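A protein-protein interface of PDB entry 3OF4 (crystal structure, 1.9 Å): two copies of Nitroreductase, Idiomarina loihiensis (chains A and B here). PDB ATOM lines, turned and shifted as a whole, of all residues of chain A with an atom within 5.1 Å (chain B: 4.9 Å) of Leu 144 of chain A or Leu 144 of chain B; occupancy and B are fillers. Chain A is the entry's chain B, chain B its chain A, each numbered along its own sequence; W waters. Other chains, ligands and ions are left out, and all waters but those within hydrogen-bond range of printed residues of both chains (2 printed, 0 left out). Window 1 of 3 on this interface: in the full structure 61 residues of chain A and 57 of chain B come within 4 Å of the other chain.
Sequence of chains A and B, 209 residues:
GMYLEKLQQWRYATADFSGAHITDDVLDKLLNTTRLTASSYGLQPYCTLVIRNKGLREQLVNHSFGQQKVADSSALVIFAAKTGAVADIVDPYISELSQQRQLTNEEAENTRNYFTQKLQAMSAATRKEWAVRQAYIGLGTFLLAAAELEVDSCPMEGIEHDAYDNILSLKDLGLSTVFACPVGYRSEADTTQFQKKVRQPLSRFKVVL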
ATOM      1  N   LEU A   4      23.571  -7.874  -6.786  1.00  0.00           N
ATOM      2  CA  LEU A   4      22.585  -7.111  -6.043  1.00  0.00           C
ATOM      3  C   LEU A   4      22.511  -7.534  -4.584  1.00  0.00           C
ATOM      4  O   LEU A   4      22.178  -6.705  -3.736  1.00  0.00           O
ATOM      5  CB  LEU A   4      21.203  -7.178  -6.715  1.00  0.00           C
ATOM      6  CG  LEU A   4      21.070  -6.242  -7.912  1.00  0.00           C
ATOM      7  CD1 LEU A   4      19.866  -6.602  -8.808  1.00  0.00           C
ATOM      8  CD2 LEU A   4      20.953  -4.810  -7.409  1.00  0.00           C
ATOM      9  N   LEU A   7      25.285  -5.662  -2.926  1.00  0.00           N
ATOM     10  CA  LEU A   7      24.816  -4.300  -2.704  1.00  0.00           C
ATOM     11  C   LEU A   7      23.858  -4.179  -1.499  1.00  0.00           C
ATOM     12  O   LEU A   7      23.941  -3.248  -0.678  1.00  0.00           O
ATOM     13  CB  LEU A   7      24.116  -3.794  -3.980  1.00  0.00           C
ATOM     14  CG  LEU A   7      24.893  -3.658  -5.293  1.00  0.00           C
ATOM     15  CD1 LEU A   7      23.981  -2.988  -6.351  1.00  0.00           C
ATOM     16  CD2 LEU A   7      26.147  -2.857  -5.067  1.00  0.00           C
ATOM     17  N   GLN A   8      22.920  -5.114  -1.385  1.00  0.00           N
ATOM     18  CA  GLN A   8      22.039  -5.165  -0.222  1.00  0.00           C
ATOM     19  C   GLN A   8      22.764  -5.252   1.121  1.00  0.00           C
ATOM     20  O   GLN A   8      22.297  -4.673   2.100  1.00  0.00           O
ATOM     21  CB  GLN A   8      21.085  -6.351  -0.338  1.00  0.00           C
ATOM     22  CG  GLN A   8      20.055  -6.200  -1.482  1.00  0.00           C
ATOM     23  CD  GLN A   8      18.867  -5.405  -1.064  1.00  0.00           C
ATOM     24  OE1 GLN A   8      18.996  -4.351  -0.415  1.00  0.00           O
ATOM     25  NE2 GLN A   8      17.678  -5.886  -1.445  1.00  0.00           N
ATOM     26  N   LEU A 139      12.239   4.257  -4.702  1.00  0.00           N
ATOM     27  CA  LEU A 139      13.107   4.166  -3.546  1.00  0.00           C
ATOM     28  C   LEU A 139      13.900   2.862  -3.564  1.00  0.00           C
ATOM     29  O   LEU A 139      15.093   2.856  -3.279  1.00  0.00           O
ATOM     30  CB  LEU A 139      12.322   4.274  -2.251  1.00  0.00           C
ATOM     31  CG  LEU A 139      13.095   4.102  -0.939  1.00  0.00           C
ATOM     32  CD1 LEU A 139      14.220   5.137  -0.798  1.00  0.00           C
ATOM     33  CD2 LEU A 139      12.136   4.210   0.224  1.00  0.00           C
ATOM     34  N   GLY A 140      13.242   1.780  -3.935  1.00  0.00           N
ATOM     35  CA  GLY A 140      13.919   0.489  -4.056  1.00  0.00           C
ATOM     36  C   GLY A 140      15.103   0.541  -5.010  1.00  0.00           C
ATOM     37  O   GLY A 140      16.217   0.060  -4.692  1.00  0.00           O
ATOM     38  N   THR A 141      14.882   1.104  -6.190  1.00  0.00           N
ATOM     39  CA  THR A 141      15.982   1.340  -7.126  1.00  0.00           C
ATOM     40  C   THR A 141      17.085   2.215  -6.507  1.00  0.00           C
ATOM     41  O   THR A 141      18.296   1.892  -6.550  1.00  0.00           O
ATOM     42  CB  THR A 141      15.476   2.005  -8.418  1.00  0.00           C
ATOM     43  OG1 THR A 141      14.487   1.181  -9.035  1.00  0.00           O
ATOM     44  CG2 THR A 141      16.637   2.216  -9.429  1.00  0.00           C
ATOM     45  N   PHE A 142      16.665   3.321  -5.932  1.00  0.00           N
ATOM     46  CA  PHE A 142      17.569   4.331  -5.392  1.00  0.00           C
ATOM     47  C   PHE A 142      18.502   3.743  -4.351  1.00  0.00           C
ATOM     48  O   PHE A 142      19.727   3.990  -4.373  1.00  0.00           O
ATOM     49  CB  PHE A 142      16.710   5.464  -4.809  1.00  0.00           C
ATOM     50  CG  PHE A 142      17.478   6.571  -4.162  1.00  0.00           C
ATOM     51  CD1 PHE A 142      17.866   6.473  -2.836  1.00  0.00           C
ATOM     52  CD2 PHE A 142      17.676   7.757  -4.831  1.00  0.00           C
ATOM     53  CE1 PHE A 142      18.510   7.528  -2.188  1.00  0.00           C
ATOM     54  CE2 PHE A 142      18.321   8.828  -4.191  1.00  0.00           C
ATOM     55  CZ  PHE A 142      18.750   8.701  -2.869  1.00  0.00           C
ATOM     56  N   LEU A 143      17.952   2.941  -3.447  1.00  0.00           N
ATOM     57  CA  LEU A 143      18.790   2.332  -2.384  1.00  0.00           C
ATOM     58  C   LEU A 143      19.898   1.434  -2.948  1.00  0.00           C
ATOM     59  O   LEU A 143      21.006   1.409  -2.433  1.00  0.00           O
ATOM     60  CB  LEU A 143      17.927   1.554  -1.409  1.00  0.00           C
ATOM     61  CG  LEU A 143      16.963   2.393  -0.585  1.00  0.00           C
ATOM     62  CD1 LEU A 143      16.029   1.498   0.163  1.00  0.00           C
ATOM     63  CD2 LEU A 143      17.707   3.364   0.329  1.00  0.00           C
ATOM     64  N   LEU A 144      19.591   0.690  -4.001  1.00  0.00           N
ATOM     65  CA  LEU A 144      20.600  -0.146  -4.678  1.00  0.00           C
ATOM     66  C   LEU A 144      21.542   0.683  -5.525  1.00  0.00           C
ATOM     67  O   LEU A 144      22.744   0.408  -5.562  1.00  0.00           O
ATOM     68  CB  LEU A 144      19.949  -1.243  -5.522  1.00  0.00           C
ATOM     69  CG  LEU A 144      19.142  -2.263  -4.695  1.00  0.00           C
ATOM     70  CD1 LEU A 144      18.242  -3.100  -5.628  1.00  0.00           C
ATOM     71  CD2 LEU A 144      20.077  -3.137  -3.887  1.00  0.00           C
ATOM     72  N   ALA A 145      21.043   1.709  -6.171  1.00  0.00           N
ATOM     73  CA  ALA A 145      21.910   2.576  -6.998  1.00  0.00           C
ATOM     74  C   ALA A 145      22.941   3.303  -6.128  1.00  0.00           C
ATOM     75  O   ALA A 145      24.149   3.380  -6.477  1.00  0.00           O
ATOM     76  CB  ALA A 145      21.078   3.563  -7.820  1.00  0.00           C
ATOM     77  N   ALA A 146      22.492   3.721  -4.944  1.00  0.00           N
ATOM     78  CA  ALA A 146      23.373   4.355  -3.987  1.00  0.00           C
ATOM     79  C   ALA A 146      24.453   3.342  -3.536  1.00  0.00           C
ATOM     80  O   ALA A 146      25.642   3.664  -3.518  1.00  0.00           O
ATOM     81  CB  ALA A 146      22.581   4.903  -2.816  1.00  0.00           C
ATOM     82  N   ALA A 147      24.049   2.093  -3.262  1.00  0.00           N
ATOM     83  CA  ALA A 147      25.021   1.083  -2.894  1.00  0.00           C
ATOM     84  C   ALA A 147      26.042   0.853  -4.024  1.00  0.00           C
ATOM     85  O   ALA A 147      27.253   0.701  -3.759  1.00  0.00           O
ATOM     86  CB  ALA A 147      24.303  -0.235  -2.503  1.00  0.00           C
ATOM     87  N   GLU A 148      25.604   0.788  -5.277  1.00  0.00           N
ATOM     88  CA  GLU A 148      26.572   0.576  -6.374  1.00  0.00           C
ATOM     89  C   GLU A 148      27.631   1.701  -6.437  1.00  0.00           C
ATOM     90  O   GLU A 148      28.798   1.443  -6.724  1.00  0.00           O
ATOM     91  CB  GLU A 148      25.894   0.440  -7.751  1.00  0.00           C
ATOM     92  CG  GLU A 148      26.924   0.283  -8.900  1.00  0.00           C
ATOM     93  CD  GLU A 148      26.360  -0.008 -10.273  1.00  0.00           C
ATOM     94  OE1 GLU A 148      25.125  -0.129 -10.466  1.00  0.00           O
ATOM     95  OE2 GLU A 148      27.189  -0.071 -11.192  1.00  0.00           O
ATOM     96  N   LEU B   4      23.600  -1.178 -12.752  1.00  0.00           N
ATOM     97  CA  LEU B   4      22.170  -1.083 -12.501  1.00  0.00           C
ATOM     98  C   LEU B   4      21.453  -0.345 -13.630  1.00  0.00           C
ATOM     99  O   LEU B   4      20.295  -0.623 -13.904  1.00  0.00           O
ATOM    100  CB  LEU B   4      21.904  -0.415 -11.142  1.00  0.00           C
ATOM    101  CG  LEU B   4      22.174  -1.329  -9.949  1.00  0.00           C
ATOM    102  CD1 LEU B   4      22.233  -0.532  -8.644  1.00  0.00           C
ATOM    103  CD2 LEU B   4      21.097  -2.425  -9.883  1.00  0.00           C
ATOM    104  N   LEU B   7      20.883  -3.069 -16.198  1.00  0.00           N
ATOM    105  CA  LEU B   7      19.761  -3.933 -15.765  1.00  0.00           C
ATOM    106  C   LEU B   7      18.447  -3.244 -16.106  1.00  0.00           C
ATOM    107  O   LEU B   7      17.497  -3.885 -16.626  1.00  0.00           O
ATOM    108  CB  LEU B   7      19.845  -4.253 -14.288  1.00  0.00           C
ATOM    109  CG  LEU B   7      21.094  -4.985 -13.774  1.00  0.00           C
ATOM    110  CD1 LEU B   7      20.934  -5.296 -12.251  1.00  0.00           C
ATOM    111  CD2 LEU B   7      21.376  -6.242 -14.590  1.00  0.00           C
ATOM    112  N   GLN B   8      18.367  -1.931 -15.833  1.00  0.00           N
ATOM    113  CA  GLN B   8      17.161  -1.143 -16.148  1.00  0.00           C
ATOM    114  C   GLN B   8      16.795  -1.146 -17.621  1.00  0.00           C
ATOM    115  O   GLN B   8      15.615  -1.118 -17.980  1.00  0.00           O
ATOM    116  CB  GLN B   8      17.319   0.340 -15.741  1.00  0.00           C
ATOM    117  CG  GLN B   8      17.382   0.588 -14.259  1.00  0.00           C
ATOM    118  CD  GLN B   8      16.013   0.621 -13.588  1.00  0.00           C
ATOM    119  OE1 GLN B   8      15.155  -0.227 -13.850  1.00  0.00           O
ATOM    120  NE2 GLN B   8      15.821   1.598 -12.678  1.00  0.00           N
ATOM    121  N   GLY B 140      10.704  -2.740  -6.374  1.00  0.00           N
ATOM    122  CA  GLY B 140      11.842  -2.075  -6.987  1.00  0.00           C
ATOM    123  C   GLY B 140      13.049  -2.990  -6.967  1.00  0.00           C
ATOM    124  O   GLY B 140      13.753  -3.147  -7.983  1.00  0.00           O
ATOM    125  N   THR B 141      13.309  -3.627  -5.835  1.00  0.00           N
ATOM    126  CA  THR B 141      14.407  -4.580  -5.778  1.00  0.00           C
ATOM    127  C   THR B 141      14.170  -5.762  -6.718  1.00  0.00           C
ATOM    128  O   THR B 141      15.080  -6.184  -7.480  1.00  0.00           O
ATOM    129  CB  THR B 141      14.601  -5.128  -4.377  1.00  0.00           C
ATOM    130  OG1 THR B 141      14.803  -4.048  -3.465  1.00  0.00           O
ATOM    131  CG2 THR B 141      15.759  -6.209  -4.310  1.00  0.00           C
ATOM    132  N   PHE B 142      12.971  -6.312  -6.654  1.00  0.00           N
ATOM    133  CA  PHE B 142      12.623  -7.543  -7.412  1.00  0.00           C
ATOM    134  C   PHE B 142      12.816  -7.343  -8.939  1.00  0.00           C
ATOM    135  O   PHE B 142      13.350  -8.212  -9.642  1.00  0.00           O
ATOM    136  CB  PHE B 142      11.171  -7.883  -7.061  1.00  0.00           C
ATOM    137  CG  PHE B 142      10.576  -9.074  -7.787  1.00  0.00           C
ATOM    138  CD1 PHE B 142       9.937  -8.893  -9.012  1.00  0.00           C
ATOM    139  CD2 PHE B 142      10.567 -10.313  -7.205  1.00  0.00           C
ATOM    140  CE1 PHE B 142       9.340  -9.966  -9.683  1.00  0.00           C
ATOM    141  CE2 PHE B 142       9.974 -11.422  -7.858  1.00  0.00           C
ATOM    142  CZ  PHE B 142       9.367 -11.242  -9.104  1.00  0.00           C
ATOM    143  N   LEU B 143      12.423  -6.190  -9.457  1.00  0.00           N
ATOM    144  CA  LEU B 143      12.553  -5.896 -10.887  1.00  0.00           C
ATOM    145  C   LEU B 143      14.027  -5.906 -11.343  1.00  0.00           C
ATOM    146  O   LEU B 143      14.355  -6.507 -12.372  1.00  0.00           O
ATOM    147  CB  LEU B 143      11.853  -4.575 -11.243  1.00  0.00           C
ATOM    148  CG  LEU B 143      10.302  -4.558 -11.113  1.00  0.00           C
ATOM    149  CD1 LEU B 143       9.829  -3.134 -11.355  1.00  0.00           C
ATOM    150  CD2 LEU B 143       9.592  -5.578 -12.060  1.00  0.00           C
ATOM    151  N   LEU B 144      14.914  -5.306 -10.553  1.00  0.00           N
ATOM    152  CA  LEU B 144      16.340  -5.349 -10.818  1.00  0.00           C
ATOM    153  C   LEU B 144      17.004  -6.740 -10.600  1.00  0.00           C
ATOM    154  O   LEU B 144      17.884  -7.129 -11.376  1.00  0.00           O
ATOM    155  CB  LEU B 144      17.062  -4.288  -9.999  1.00  0.00           C
ATOM    156  CG  LEU B 144      16.667  -2.840 -10.319  1.00  0.00           C
ATOM    157  CD1 LEU B 144      17.227  -1.917  -9.260  1.00  0.00           C
ATOM    158  CD2 LEU B 144      17.146  -2.443 -11.704  1.00  0.00           C
ATOM    159  N   ALA B 145      16.594  -7.445  -9.556  1.00  0.00           N
ATOM    160  CA  ALA B 145      17.076  -8.792  -9.288  1.00  0.00           C
ATOM    161  C   ALA B 145      16.709  -9.719 -10.434  1.00  0.00           C
ATOM    162  O   ALA B 145      17.516 -10.532 -10.855  1.00  0.00           O
ATOM    163  CB  ALA B 145      16.470  -9.317  -8.006  1.00  0.00           C
ATOM    164  N   ALA B 146      15.483  -9.601 -10.926  1.00  0.00           N
ATOM    165  CA  ALA B 146      15.045 -10.379 -12.090  1.00  0.00           C
ATOM    166  C   ALA B 146      15.936 -10.083 -13.286  1.00  0.00           C
ATOM    167  O   ALA B 146      16.392 -11.017 -13.947  1.00  0.00           O
ATOM    168  CB  ALA B 146      13.547 -10.085 -12.445  1.00  0.00           C
ATOM    169  N   ALA B 147      16.191  -8.787 -13.545  1.00  0.00           N
ATOM    170  CA  ALA B 147      17.072  -8.348 -14.624  1.00  0.00           C
ATOM    171  C   ALA B 147      18.453  -8.957 -14.493  1.00  0.00           C
ATOM    172  O   ALA B 147      19.010  -9.492 -15.459  1.00  0.00           O
ATOM    173  CB  ALA B 147      17.171  -6.822 -14.664  1.00  0.00           C
ATOM    174  N   GLU B 148      19.026  -8.891 -13.296  1.00  0.00           N
ATOM    175  CA  GLU B 148      20.348  -9.482 -13.113  1.00  0.00           C
ATOM    176  C   GLU B 148      20.324 -10.977 -13.500  1.00  0.00           C
ATOM    177  O   GLU B 148      21.243 -11.480 -14.153  1.00  0.00           O
ATOM    178  CB  GLU B 148      20.875  -9.281 -11.683  1.00  0.00           C
ATOM    179  CG  GLU B 148      22.158 -10.121 -11.464  1.00  0.00           C
ATOM    180  CD  GLU B 148      22.893  -9.854 -10.157  1.00  0.00           C
ATOM    181  OE1 GLU B 148      22.422  -9.091  -9.293  1.00  0.00           O
ATOM    182  OE2 GLU B 148      23.991 -10.423 -10.012  1.00  0.00           O
HETATM  183  O   HOH W   1      16.233  -1.714  -2.560  1.00  0.00           O
HETATM  184  O   HOH W   2      13.354  -1.179  -9.947  1.00  0.00           O
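The backbone NH (N) of Leu 4 of chain B lies within hydrogen-bond range of the side-chain carboxylate (OE1) of Glu 148 of chain A (2.9 Å).
N of Leu 4 of chain A sits at hydrogen-bond distance from OE1 of Glu 148 of chain B, at 3.0 Å.
CD2 of Leu 4 of chain B touches CD2 of Leu 4 of chain A, at 3.4 Å.
CD1 of Leu 4 of chain A touches CD1 of Leu 7 of chain B, 3.8 Å away.
O of Leu 144 of chain B touches CD1 of Leu 4 of chain A, 3.3 Å away.
Leu 4 of chain A touches Ala 145 of chain B (CD1 to N, 3.5 Å).
Leu 4 of chain B touches Leu 7 of chain A (CD1 to CD1, 3.8 Å).
Thr 141 of chain B touches Gln 8 of chain A (CG2 to NE2, 3.5 Å).
Gln 8 of chain B touches Thr 141 of chain A (NE2 to CG2, 3.4 Å).
Leu 144 of chain A touches Leu 4 of chain B.
CD1 of Leu 144 of chain A touches CD1 of Leu 144 of chain B, 3.95 Å away.
Leu 4 of chain B touches Ala 145 of chain A.
Of the printed residues of chain B, Leu 144 of chain A touches Leu 4 and Leu 144.
Of the printed residues of chain A, Leu 144 of chain B touches Leu 4 and Leu 144.
Of the printed residues of chain B, Thr 141 of chain A touches Gln 8 (3.4 Å).
Of the printed residues of chain A, Gln 8 of chain B touches Thr 141 (3.4 Å).
Of the printed residues of chain A, Ala 145 of chain B touches Leu 4 (3.5 Å).
Of the printed residues of chain B, Gln 8 of chain A touches Thr 141.
Hydrophobic or aromatic side chains of chain A that line the printed part of chain B: Leu 4, Leu 7 and Leu 144.
Leu 4 of chain B touches its own counterpart, Leu 4 of chain A.
Leu 4 of chain A touches Leu 144 of chain B, and with the chains exchanged Leu 144 of chain A touches Leu 4 of chain B.
Leu 4 of chain A touches Glu 148 of chain B, and with the chains exchanged Glu 148 of chain A touches Leu 4 of chain B.
Gln 8 of chain A touches Thr 141 of chain B, and with the chains exchanged Thr 141 of chain A touches Gln 8 of chain B.
12 positions are printed for both chains.
Water W2 bridges the side-chain hydroxyl of Thr 141 of chain A (2.8 Å) and the backbone carbonyl oxygen of Gly 140 of chain B (2.8 Å).
Water W1 bridges the backbone carbonyl oxygen of Gly 140 of chain A (2.8 Å) and the side-chain hydroxyl of Thr 141 of chain B (2.9 Å).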
